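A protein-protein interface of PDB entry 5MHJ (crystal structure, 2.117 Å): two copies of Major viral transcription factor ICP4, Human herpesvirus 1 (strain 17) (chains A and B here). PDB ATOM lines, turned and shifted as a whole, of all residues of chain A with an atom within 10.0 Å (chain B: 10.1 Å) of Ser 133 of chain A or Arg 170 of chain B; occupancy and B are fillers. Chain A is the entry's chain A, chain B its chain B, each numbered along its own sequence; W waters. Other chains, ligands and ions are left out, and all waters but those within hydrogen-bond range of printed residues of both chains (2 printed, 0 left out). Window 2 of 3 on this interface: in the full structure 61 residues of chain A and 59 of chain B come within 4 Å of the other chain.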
ATOM      1  N   GLY A  44     -23.734  30.333 -33.618  1.00  0.00           N
ATOM      2  CA  GLY A  44     -22.423  30.373 -33.003  1.00  0.00           C
ATOM      3  C   GLY A  44     -22.172  31.612 -32.166  1.00  0.00           C
ATOM      4  O   GLY A  44     -23.059  32.069 -31.436  1.00  0.00           O
ATOM      5  N   GLY A  45     -20.966  32.161 -32.265  1.00  0.00           N
ATOM      6  CA  GLY A  45     -20.574  33.307 -31.475  1.00  0.00           C
ATOM      7  C   GLY A  45     -21.182  34.599 -31.987  1.00  0.00           C
ATOM      8  O   GLY A  45     -22.044  34.621 -32.868  1.00  0.00           O
ATOM      9  N   PHE A 122     -26.018  21.959 -37.828  1.00  0.00           N
ATOM     10  CA  PHE A 122     -24.565  21.945 -37.696  1.00  0.00           C
ATOM     11  C   PHE A 122     -23.888  21.558 -39.002  1.00  0.00           C
ATOM     12  O   PHE A 122     -22.778  22.028 -39.285  1.00  0.00           O
ATOM     13  CB  PHE A 122     -24.134  20.987 -36.584  1.00  0.00           C
ATOM     14  CG  PHE A 122     -22.650  20.986 -36.337  1.00  0.00           C
ATOM     15  CD1 PHE A 122     -22.089  21.872 -35.432  1.00  0.00           C
ATOM     16  CD2 PHE A 122     -21.815  20.114 -37.019  1.00  0.00           C
ATOM     17  CE1 PHE A 122     -20.725  21.885 -35.206  1.00  0.00           C
ATOM     18  CE2 PHE A 122     -20.449  20.124 -36.799  1.00  0.00           C
ATOM     19  CZ  PHE A 122     -19.904  21.011 -35.894  1.00  0.00           C
ATOM     20  N   ALA A 127     -18.653  23.931 -39.532  1.00  0.00           N
ATOM     21  CA  ALA A 127     -17.728  23.793 -38.419  1.00  0.00           C
ATOM     22  C   ALA A 127     -17.082  22.412 -38.434  1.00  0.00           C
ATOM     23  O   ALA A 127     -17.662  21.432 -38.911  1.00  0.00           O
ATOM     24  CB  ALA A 127     -18.448  24.027 -37.091  1.00  0.00           C
ATOM     25  N   ARG A 129     -15.736  20.272 -35.739  1.00  0.00           N
ATOM     26  CA  ARG A 129     -16.175  19.274 -34.773  1.00  0.00           C
ATOM     27  C   ARG A 129     -17.359  19.802 -33.977  1.00  0.00           C
ATOM     28  O   ARG A 129     -17.337  20.945 -33.507  1.00  0.00           O
ATOM     29  CB  ARG A 129     -15.034  18.898 -33.822  1.00  0.00           C
ATOM     30  CG  ARG A 129     -13.926  18.081 -34.462  1.00  0.00           C
ATOM     31  CD  ARG A 129     -14.279  16.604 -34.495  1.00  0.00           C
ATOM     32  NE  ARG A 129     -13.170  15.789 -34.984  1.00  0.00           N
ATOM     33  CZ  ARG A 129     -12.158  15.372 -34.229  1.00  0.00           C
ATOM     34  NH1 ARG A 129     -12.111  15.692 -32.943  1.00  0.00           N
ATOM     35  NH2 ARG A 129     -11.192  14.634 -34.760  1.00  0.00           N
ATOM     36  N   ASN A 130     -18.388  18.971 -33.832  1.00  0.00           N
ATOM     37  CA  ASN A 130     -19.479  19.244 -32.907  1.00  0.00           C
ATOM     38  C   ASN A 130     -19.168  18.567 -31.581  1.00  0.00           C
ATOM     39  O   ASN A 130     -18.756  17.403 -31.554  1.00  0.00           O
ATOM     40  CB  ASN A 130     -20.816  18.744 -33.456  1.00  0.00           C
ATOM     41  CG  ASN A 130     -22.003  19.329 -32.711  1.00  0.00           C
ATOM     42  OD1 ASN A 130     -21.854  20.266 -31.924  1.00  0.00           O
ATOM     43  ND2 ASN A 130     -23.188  18.780 -32.956  1.00  0.00           N
ATOM     44  N   SER A 131     -19.361  19.294 -30.488  1.00  0.00           N
ATOM     45  CA  SER A 131     -19.000  18.782 -29.174  1.00  0.00           C
ATOM     46  C   SER A 131     -19.736  19.584 -28.112  1.00  0.00           C
ATOM     47  O   SER A 131     -20.507  20.499 -28.414  1.00  0.00           O
ATOM     48  CB  SER A 131     -17.488  18.843 -28.961  1.00  0.00           C
ATOM     49  OG  SER A 131     -17.035  20.184 -28.873  1.00  0.00           O
ATOM     50  N   SER A 132     -19.484  19.228 -26.852  1.00  0.00           N
ATOM     51  CA  SER A 132     -20.018  19.997 -25.738  1.00  0.00           C
ATOM     52  C   SER A 132     -19.377  21.373 -25.633  1.00  0.00           C
ATOM     53  O   SER A 132     -19.924  22.248 -24.953  1.00  0.00           O
ATOM     54  CB  SER A 132     -19.821  19.227 -24.433  1.00  0.00           C
ATOM     55  OG  SER A 132     -20.550  18.011 -24.446  1.00  0.00           O
ATOM     56  N   SER A 133     -18.240  21.583 -26.297  1.00  0.00           N
ATOM     57  CA  SER A 133     -17.494  22.830 -26.209  1.00  0.00           C
ATOM     58  C   SER A 133     -17.845  23.816 -27.314  1.00  0.00           C
ATOM     59  O   SER A 133     -17.424  24.976 -27.243  1.00  0.00           O
ATOM     60  CB  SER A 133     -15.989  22.546 -26.261  1.00  0.00           C
ATOM     61  OG  SER A 133     -15.666  21.352 -25.571  1.00  0.00           O
ATOM     62  N   PHE A 134     -18.583  23.383 -28.331  1.00  0.00           N
ATOM     63  CA  PHE A 134     -18.887  24.249 -29.462  1.00  0.00           C
ATOM     64  C   PHE A 134     -19.808  25.379 -29.021  1.00  0.00           C
ATOM     65  O   PHE A 134     -20.876  25.137 -28.450  1.00  0.00           O
ATOM     66  CB  PHE A 134     -19.523  23.441 -30.589  1.00  0.00           C
ATOM     67  CG  PHE A 134     -19.748  24.232 -31.843  1.00  0.00           C
ATOM     68  CD1 PHE A 134     -18.675  24.709 -32.578  1.00  0.00           C
ATOM     69  CD2 PHE A 134     -21.030  24.502 -32.287  1.00  0.00           C
ATOM     70  CE1 PHE A 134     -18.878  25.438 -33.733  1.00  0.00           C
ATOM     71  CE2 PHE A 134     -21.241  25.230 -33.440  1.00  0.00           C
ATOM     72  CZ  PHE A 134     -20.163  25.700 -34.164  1.00  0.00           C
ATOM     73  N   ILE A 135     -19.387  26.615 -29.279  1.00  0.00           N
ATOM     74  CA  ILE A 135     -20.196  27.778 -28.936  1.00  0.00           C
ATOM     75  C   ILE A 135     -21.343  27.883 -29.931  1.00  0.00           C
ATOM     76  O   ILE A 135     -21.125  28.044 -31.137  1.00  0.00           O
ATOM     77  CB  ILE A 135     -19.345  29.053 -28.922  1.00  0.00           C
ATOM     78  CG1 ILE A 135     -18.353  29.013 -27.757  1.00  0.00           C
ATOM     79  CG2 ILE A 135     -20.234  30.286 -28.848  1.00  0.00           C
ATOM     80  CD1 ILE A 135     -17.432  30.210 -27.692  1.00  0.00           C
ATOM     81  N   THR A 136     -22.574  27.786 -29.430  1.00  0.00           N
ATOM     82  CA  THR A 136     -23.750  27.802 -30.285  1.00  0.00           C
ATOM     83  C   THR A 136     -24.594  29.057 -30.143  1.00  0.00           C
ATOM     84  O   THR A 136     -25.401  29.339 -31.033  1.00  0.00           O
ATOM     85  CB  THR A 136     -24.638  26.583 -29.995  1.00  0.00           C
ATOM     86  OG1 THR A 136     -25.133  26.666 -28.653  1.00  0.00           O
ATOM     87  CG2 THR A 136     -23.848  25.296 -30.159  1.00  0.00           C
ATOM     88  N   GLY A 137     -24.434  29.811 -29.059  1.00  0.00           N
ATOM     89  CA  GLY A 137     -25.279  30.957 -28.810  1.00  0.00           C
ATOM     90  C   GLY A 137     -26.573  30.650 -28.092  1.00  0.00           C
ATOM     91  O   GLY A 137     -27.381  31.568 -27.891  1.00  0.00           O
ATOM     92  N   SER A 138     -26.803  29.393 -27.707  1.00  0.00           N
ATOM     93  CA  SER A 138     -27.979  29.021 -26.921  1.00  0.00           C
ATOM     94  C   SER A 138     -27.688  27.717 -26.195  1.00  0.00           C
ATOM     95  O   SER A 138     -27.344  26.720 -26.838  1.00  0.00           O
ATOM     96  CB  SER A 138     -29.213  28.878 -27.807  1.00  0.00           C
ATOM     97  OG  SER A 138     -30.360  28.591 -27.021  1.00  0.00           O
ATOM     98  N   VAL A 139     -27.841  27.716 -24.868  1.00  0.00           N
ATOM     99  CA  VAL A 139     -27.525  26.520 -24.090  1.00  0.00           C
ATOM    100  C   VAL A 139     -28.601  25.450 -24.262  1.00  0.00           C
ATOM    101  O   VAL A 139     -28.324  24.253 -24.114  1.00  0.00           O
ATOM    102  CB  VAL A 139     -27.309  26.886 -22.606  1.00  0.00           C
ATOM    103  CG1 VAL A 139     -28.608  27.354 -21.954  1.00  0.00           C
ATOM    104  CG2 VAL A 139     -26.709  25.709 -21.843  1.00  0.00           C
ATOM    105  N   ALA A 140     -29.829  25.848 -24.585  1.00  0.00           N
ATOM    106  CA  ALA A 140     -30.918  24.918 -24.861  1.00  0.00           C
ATOM    107  C   ALA A 140     -31.403  25.148 -26.284  1.00  0.00           C
ATOM    108  O   ALA A 140     -31.639  26.293 -26.682  1.00  0.00           O
ATOM    109  CB  ALA A 140     -32.068  25.094 -23.865  1.00  0.00           C
ATOM    110  N   ALA A 165     -29.837  27.964 -18.751  1.00  0.00           N
ATOM    111  CA  ALA A 165     -28.527  27.653 -18.182  1.00  0.00           C
ATOM    112  C   ALA A 165     -28.664  26.956 -16.836  1.00  0.00           C
ATOM    113  O   ALA A 165     -27.978  25.962 -16.568  1.00  0.00           O
ATOM    114  CB  ALA A 165     -27.695  28.927 -18.039  1.00  0.00           C
ATOM    115  N   MET A 168     -30.088  23.424 -17.474  1.00  0.00           N
ATOM    116  CA  MET A 168     -29.135  22.502 -18.083  1.00  0.00           C
ATOM    117  C   MET A 168     -28.023  22.077 -17.133  1.00  0.00           C
ATOM    118  O   MET A 168     -27.364  21.063 -17.392  1.00  0.00           O
ATOM    119  CB  MET A 168     -28.524  23.134 -19.337  1.00  0.00           C
ATOM    120  CG  MET A 168     -29.463  23.130 -20.525  1.00  0.00           C
ATOM    121  SD  MET A 168     -29.817  21.458 -21.082  1.00  0.00           S
ATOM    122  CE  MET A 168     -28.209  20.933 -21.668  1.00  0.00           C
ATOM    123  N   SER A 169     -27.797  22.817 -16.051  1.00  0.00           N
ATOM    124  CA  SER A 169     -26.718  22.483 -15.130  1.00  0.00           C
ATOM    125  C   SER A 169     -27.018  21.194 -14.372  1.00  0.00           C
ATOM    126  O   SER A 169     -28.152  20.946 -13.957  1.00  0.00           O
ATOM    127  CB  SER A 169     -26.496  23.623 -14.135  1.00  0.00           C
ATOM    128  OG  SER A 169     -25.499  23.274 -13.190  1.00  0.00           O
ATOM    129  N   GLN B 106     -15.960  31.743 -13.566  1.00  0.00           N
ATOM    130  CA  GLN B 106     -15.642  30.534 -14.317  1.00  0.00           C
ATOM    131  C   GLN B 106     -14.229  30.040 -14.029  1.00  0.00           C
ATOM    132  O   GLN B 106     -14.014  28.832 -13.876  1.00  0.00           O
ATOM    133  CB  GLN B 106     -15.820  30.786 -15.813  1.00  0.00           C
ATOM    134  CG  GLN B 106     -15.486  29.590 -16.686  1.00  0.00           C
ATOM    135  CD  GLN B 106     -15.820  29.830 -18.141  1.00  0.00           C
ATOM    136  OE1 GLN B 106     -15.922  30.975 -18.585  1.00  0.00           O
ATOM    137  NE2 GLN B 106     -16.004  28.752 -18.894  1.00  0.00           N
ATOM    138  N   ASN B 107     -13.259  30.949 -13.959  1.00  0.00           N
ATOM    139  CA  ASN B 107     -11.853  30.590 -13.770  1.00  0.00           C
ATOM    140  C   ASN B 107     -11.204  31.578 -12.815  1.00  0.00           C
ATOM    141  O   ASN B 107     -10.516  32.517 -13.234  1.00  0.00           O
ATOM    142  CB  ASN B 107     -11.107  30.557 -15.106  1.00  0.00           C
ATOM    143  CG  ASN B 107     -11.358  29.283 -15.880  1.00  0.00           C
ATOM    144  OD1 ASN B 107     -11.993  29.297 -16.933  1.00  0.00           O
ATOM    145  ND2 ASN B 107     -10.857  28.167 -15.359  1.00  0.00           N
ATOM    146  N   VAL B 139     -23.101  26.050  -8.640  1.00  0.00           N
ATOM    147  CA  VAL B 139     -22.362  25.786  -9.867  1.00  0.00           C
ATOM    148  C   VAL B 139     -20.986  26.452  -9.854  1.00  0.00           C
ATOM    149  O   VAL B 139     -20.091  26.018 -10.587  1.00  0.00           O
ATOM    150  CB  VAL B 139     -23.216  26.207 -11.083  1.00  0.00           C
ATOM    151  CG1 VAL B 139     -23.345  27.715 -11.169  1.00  0.00           C
ATOM    152  CG2 VAL B 139     -22.647  25.625 -12.369  1.00  0.00           C
ATOM    153  N   ALA B 164     -23.656  32.665 -12.404  1.00  0.00           N
ATOM    154  CA  ALA B 164     -22.602  31.657 -12.420  1.00  0.00           C
ATOM    155  C   ALA B 164     -22.943  30.498 -13.348  1.00  0.00           C
ATOM    156  O   ALA B 164     -22.043  29.918 -13.965  1.00  0.00           O
ATOM    157  CB  ALA B 164     -22.338  31.145 -11.005  1.00  0.00           C
ATOM    158  N   ALA B 165     -24.228  30.147 -13.459  1.00  0.00           N
ATOM    159  CA  ALA B 165     -24.628  29.114 -14.408  1.00  0.00           C
ATOM    160  C   ALA B 165     -24.331  29.543 -15.838  1.00  0.00           C
ATOM    161  O   ALA B 165     -23.824  28.751 -16.642  1.00  0.00           O
ATOM    162  CB  ALA B 165     -26.113  28.790 -14.241  1.00  0.00           C
ATOM    163  N   VAL B 166     -24.638  30.799 -16.172  1.00  0.00           N
ATOM    164  CA  VAL B 166     -24.315  31.317 -17.495  1.00  0.00           C
ATOM    165  C   VAL B 166     -22.806  31.347 -17.705  1.00  0.00           C
ATOM    166  O   VAL B 166     -22.308  30.974 -18.773  1.00  0.00           O
ATOM    167  CB  VAL B 166     -24.940  32.712 -17.685  1.00  0.00           C
ATOM    168  CG1 VAL B 166     -24.400  33.370 -18.951  1.00  0.00           C
ATOM    169  CG2 VAL B 166     -26.460  32.611 -17.732  1.00  0.00           C
ATOM    170  N   ALA B 167     -22.053  31.779 -16.687  1.00  0.00           N
ATOM    171  CA  ALA B 167     -20.603  31.880 -16.827  1.00  0.00           C
ATOM    172  C   ALA B 167     -19.956  30.519 -17.035  1.00  0.00           C
ATOM    173  O   ALA B 167     -18.952  30.413 -17.749  1.00  0.00           O
ATOM    174  CB  ALA B 167     -20.000  32.569 -15.602  1.00  0.00           C
ATOM    175  N   MET B 168     -20.509  29.469 -16.426  1.00  0.00           N
ATOM    176  CA  MET B 168     -19.951  28.130 -16.559  1.00  0.00           C
ATOM    177  C   MET B 168     -20.373  27.429 -17.845  1.00  0.00           C
ATOM    178  O   MET B 168     -19.759  26.419 -18.203  1.00  0.00           O
ATOM    179  CB  MET B 168     -20.351  27.270 -15.357  1.00  0.00           C
ATOM    180  CG  MET B 168     -19.764  27.743 -14.038  1.00  0.00           C
ATOM    181  SD  MET B 168     -17.966  27.645 -13.997  1.00  0.00           S
ATOM    182  CE  MET B 168     -17.723  25.878 -13.857  1.00  0.00           C
ATOM    183  N   SER B 169     -21.388  27.930 -18.543  1.00  0.00           N
ATOM    184  CA  SER B 169     -21.844  27.288 -19.768  1.00  0.00           C
ATOM    185  C   SER B 169     -20.806  27.425 -20.875  1.00  0.00           C
ATOM    186  O   SER B 169     -20.107  28.436 -20.987  1.00  0.00           O
ATOM    187  CB  SER B 169     -23.170  27.889 -20.232  1.00  0.00           C
ATOM    188  OG  SER B 169     -23.545  27.369 -21.501  1.00  0.00           O
ATOM    189  N   ARG B 170     -20.715  26.390 -21.706  1.00  0.00           N
ATOM    190  CA  ARG B 170     -19.793  26.363 -22.832  1.00  0.00           C
ATOM    191  C   ARG B 170     -20.452  26.774 -24.141  1.00  0.00           C
ATOM    192  O   ARG B 170     -19.813  26.694 -25.194  1.00  0.00           O
ATOM    193  CB  ARG B 170     -19.180  24.970 -22.976  1.00  0.00           C
ATOM    194  CG  ARG B 170     -18.687  24.368 -21.673  1.00  0.00           C
ATOM    195  CD  ARG B 170     -18.014  23.029 -21.916  1.00  0.00           C
ATOM    196  NE  ARG B 170     -16.638  23.179 -22.379  1.00  0.00           N
ATOM    197  CZ  ARG B 170     -15.866  22.168 -22.760  1.00  0.00           C
ATOM    198  NH1 ARG B 170     -16.335  20.926 -22.740  1.00  0.00           N
ATOM    199  NH2 ARG B 170     -14.625  22.396 -23.167  1.00  0.00           N
ATOM    200  N   ARG B 171     -21.708  27.215 -24.101  1.00  0.00           N
ATOM    201  CA  ARG B 171     -22.456  27.517 -25.312  1.00  0.00           C
ATOM    202  C   ARG B 171     -22.459  28.996 -25.670  1.00  0.00           C
ATOM    203  O   ARG B 171     -22.960  29.356 -26.741  1.00  0.00           O
ATOM    204  CB  ARG B 171     -23.902  27.024 -25.177  1.00  0.00           C
ATOM    205  CG  ARG B 171     -24.028  25.522 -24.972  1.00  0.00           C
ATOM    206  CD  ARG B 171     -23.370  24.742 -26.104  1.00  0.00           C
ATOM    207  NE  ARG B 171     -23.725  23.325 -26.065  1.00  0.00           N
ATOM    208  CZ  ARG B 171     -23.177  22.392 -26.836  1.00  0.00           C
ATOM    209  NH1 ARG B 171     -22.233  22.718 -27.711  1.00  0.00           N
ATOM    210  NH2 ARG B 171     -23.566  21.128 -26.729  1.00  0.00           N
ATOM    211  N   TYR B 172     -21.918  29.854 -24.810  1.00  0.00           N
ATOM    212  CA  TYR B 172     -21.851  31.286 -25.052  1.00  0.00           C
ATOM    213  C   TYR B 172     -20.401  31.745 -25.013  1.00  0.00           C
ATOM    214  O   TYR B 172     -19.604  31.240 -24.215  1.00  0.00           O
ATOM    215  CB  TYR B 172     -22.665  32.063 -24.012  1.00  0.00           C
ATOM    216  CG  TYR B 172     -24.097  31.599 -23.864  1.00  0.00           C
ATOM    217  CD1 TYR B 172     -25.053  31.928 -24.816  1.00  0.00           C
ATOM    218  CD2 TYR B 172     -24.499  30.847 -22.765  1.00  0.00           C
ATOM    219  CE1 TYR B 172     -26.366  31.514 -24.685  1.00  0.00           C
ATOM    220  CE2 TYR B 172     -25.812  30.428 -22.626  1.00  0.00           C
ATOM    221  CZ  TYR B 172     -26.741  30.765 -23.589  1.00  0.00           C
ATOM    222  OH  TYR B 172     -28.050  30.353 -23.461  1.00  0.00           O
ATOM    223  N   ASP B 173     -20.059  32.707 -25.870  1.00  0.00           N
ATOM    224  CA  ASP B 173     -18.742  33.327 -25.811  1.00  0.00           C
ATOM    225  C   ASP B 173     -18.772  34.475 -24.801  1.00  0.00           C
ATOM    226  O   ASP B 173     -19.767  34.691 -24.103  1.00  0.00           O
ATOM    227  CB  ASP B 173     -18.286  33.769 -27.204  1.00  0.00           C
ATOM    228  CG  ASP B 173     -19.186  34.829 -27.826  1.00  0.00           C
ATOM    229  OD1 ASP B 173     -20.018  35.431 -27.118  1.00  0.00           O
ATOM    230  OD2 ASP B 173     -19.054  35.063 -29.046  1.00  0.00           O
ATOM    231  N   ARG B 174     -17.676  35.235 -24.722  1.00  0.00           N
ATOM    232  CA  ARG B 174     -17.567  36.273 -23.701  1.00  0.00           C
ATOM    233  C   ARG B 174     -18.516  37.433 -23.978  1.00  0.00           C
ATOM    234  O   ARG B 174     -19.132  37.971 -23.050  1.00  0.00           O
ATOM    235  CB  ARG B 174     -16.122  36.768 -23.606  1.00  0.00           C
ATOM    236  CG  ARG B 174     -15.134  35.708 -23.131  1.00  0.00           C
ATOM    237  CD  ARG B 174     -13.791  36.320 -22.758  1.00  0.00           C
ATOM    238  NE  ARG B 174     -13.433  37.423 -23.645  1.00  0.00           N
ATOM    239  CZ  ARG B 174     -12.187  37.820 -23.883  1.00  0.00           C
ATOM    240  NH1 ARG B 174     -11.167  37.206 -23.298  1.00  0.00           N
ATOM    241  NH2 ARG B 174     -11.961  38.834 -24.708  1.00  0.00           N
ATOM    242  N   GLN B 176     -21.370  37.289 -25.590  1.00  0.00           N
ATOM    243  CA  GLN B 176     -22.726  36.839 -25.289  1.00  0.00           C
ATOM    244  C   GLN B 176     -22.973  36.817 -23.786  1.00  0.00           C
ATOM    245  O   GLN B 176     -24.046  37.222 -23.322  1.00  0.00           O
ATOM    246  CB  GLN B 176     -22.970  35.462 -25.912  1.00  0.00           C
ATOM    247  CG  GLN B 176     -23.164  35.508 -27.427  1.00  0.00           C
ATOM    248  CD  GLN B 176     -22.947  34.168 -28.100  1.00  0.00           C
ATOM    249  OE1 GLN B 176     -22.379  33.251 -27.513  1.00  0.00           O
ATOM    250  NE2 GLN B 176     -23.387  34.055 -29.348  1.00  0.00           N
ATOM    251  N   LYS B 177     -21.985  36.374 -23.006  1.00  0.00           N
ATOM    252  CA  LYS B 177     -22.127  36.387 -21.553  1.00  0.00           C
ATOM    253  C   LYS B 177     -22.216  37.808 -21.006  1.00  0.00           C
ATOM    254  O   LYS B 177     -22.891  38.038 -19.994  1.00  0.00           O
ATOM    255  CB  LYS B 177     -20.960  35.637 -20.908  1.00  0.00           C
ATOM    256  CG  LYS B 177     -21.001  34.135 -21.143  1.00  0.00           C
ATOM    257  CD  LYS B 177     -19.747  33.457 -20.622  1.00  0.00           C
ATOM    258  CE  LYS B 177     -19.836  31.948 -20.782  1.00  0.00           C
ATOM    259  NZ  LYS B 177     -18.586  31.270 -20.348  1.00  0.00           N
HETATM  260  O   HOH W   1     -22.931  19.365 -28.991  1.00  0.00           O
HETATM  261  O   HOH W   2     -26.015  22.631 -24.732  1.00  0.00           O
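The backbone NH (N) of Gly 44 of chain A lies within hydrogen-bond range of the backbone carbonyl oxygen (O) of Thr 136 of chain A.
OG of Ser 131 of chain A sits close to N of Ser 133 of chain A (3.2 Å).
The side-chain hydroxyl (OG1) of Thr 136 of chain A is in hydrogen-bond range of the backbone carbonyl oxygen (O) of Ser 138 of chain A (2.9 Å).
OG of Ser 138 of chain A is in hydrogen-bond range of O of Ala 140 of chain A, at 2.7 Å.
The side-chain amino group (NZ) of Lys 177 of chain B sits at hydrogen-bond distance from the backbone carbonyl oxygen (O) of Ser 169 of chain B, at 3.3 Å.
The side-chain carboxylate (OD1) of Asp 173 of chain B sits at hydrogen-bond distance from the backbone NH (N) of Gln 176 of chain B, 2.8 Å away.
Among the printed residues, merely in contact across the chains: Gly 45 of chain A with Asp 173 of chain B (3.4 Å), Gly 45 of chain A with Gln 176 of chain B (3.5 Å), Ser 132 of chain A with Arg 170 of chain B (3.4 Å), Ser 132 of chain A with Arg 171 of chain B (3.6 Å), Phe 134 of chain A with Arg 170 of chain B (3.8 Å), Ile 135 of chain A with Arg 170 of chain B (3.8 Å), Ile 135 of chain A with Arg 171 of chain B (3.6 Å), Ile 135 of chain A with Asp 173 of chain B (3.7 Å), Ile 135 of chain A with Gln 176 of chain B (3.9 Å), Gly 137 of chain A with Tyr 172 of chain B (3.4 Å), Gly 137 of chain A with Gln 176 of chain B (3.7 Å), Ser 138 of chain A with Arg 171 of chain B (3.8 Å), Ser 138 of chain A with Tyr 172 of chain B (3.7 Å), Val 139 of chain A with Ser 169 of chain B (3.6 Å), Val 139 of chain A with Arg 171 of chain B (3.7 Å), Ala 165 of chain A with Val 166 of chain B (3.9 Å) and Ser 169 of chain A with Val 139 of chain B (3.8 Å).
Water W1 lies within hydrogen-bond range of the backbone carbonyl oxygen (O) of Ser 131 of chain A (2.7 Å), the guanidinium group (NH2) of Arg 171 of chain B (2.9 Å) and the side-chain amide oxygen (OD1) of Asn 130 of chain A (3.3 Å).
Water W2 bridges NE of Arg 171 of chain B and O of Val 139 of chain A.
Of the 19 printed residues of chain A, 13 touch a printed residue of chain B.
Hydrophobic or aromatic side chains of chain A within 4 Å of the printed part of chain B: Ile 135, Val 139 and Ala 165.
Along chain A the printed residues that touch a printed residue of chain B span positions 44 to 169.
Among the printed residues, no Asp or Glu carboxylate lies within 4 Å of a Lys or Arg side-chain nitrogen of the other chain.
The backbone carbonyl oxygen (O) of Gly 44 of chain A is in hydrogen-bond range of the side-chain amide nitrogen (NE2) of Gln 176 of chain B, at 2.9 Å.
The guanidinium group (NH1) of Arg 171 of chain B sits at hydrogen-bond distance from the backbone carbonyl oxygen (O) of Ser 131 of chain A, 2.9 Å away.
The side-chain hydroxyl (OG) of Ser 133 of chain A is in hydrogen-bond range of the guanidinium group (NH2) of Arg 170 of chain B (2.8 Å).
The guanidinium group of Arg 171 of chain B sits at hydrogen-bond distance from the backbone carbonyl oxygen of Phe 134 of chain A (2.9 Å).
N of Thr 136 of chain A sits at hydrogen-bond distance from O of Arg 171 of chain B (3.1 Å).
The backbone carbonyl oxygen (O) of Arg 171 of chain B sits at hydrogen-bond distance from the backbone NH (N) of Gly 137 of chain A.
N of Val 139 of chain A is in hydrogen-bond range of OH of Tyr 172 of chain B.
Val 139 of chain A touches Ser 169 of chain B, and with the chains exchanged Ser 169 of chain A touches Val 139 of chain B.
Of the 24 pairs that touch across the chains among the printed residues, 2 have their exchanged pair printed and touching as well.
Of the printed residues of chain B, Gly 45 of chain A touches Asp 173 (3.4 Å) and Gln 176 (3.5 Å).
Asn 130 of chain A touches none of the printed residues of chain B.
Ser 131 of chain A touches just one residue of chain B: Arg 171 (2.9 Å).
Ser 133 of chain A touches just one residue of chain B: Arg 170 (2.8 Å).
Of the printed residues of chain A, Val 139 of chain B touches Ser 169.
Ala 165 of chain B touches none of the printed residues of chain A.
Ser 169 of chain B touches just one residue of chain A: Val 139.
Of chain A, only Ser 132, Ser 133, Phe 134 and Ile 135 come within 4 Å of Arg 170 of chain B.
Of chain A, only Ser 131 (2.9 Å), Ser 132 (3.6 Å), Phe 134 (2.9 Å), Ile 135 (3.6 Å), Thr 136 (3.1 Å), Gly 137 (2.8 Å), Ser 138 (3.8 Å) and Val 139 (3.7 Å) come within 4 Å of Arg 171 of chain B.
Of the printed residues of chain A, Tyr 172 of chain B touches Gly 137, Ser 138 and Val 139.
Of the printed residues of chain A, Gln 176 of chain B touches Gly 44, Gly 45, Ile 135 and Gly 137.
The nearest printed residue of chain A that does not touch Asp 173 of chain B is Gly 44 of chain A (5.5 Å).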
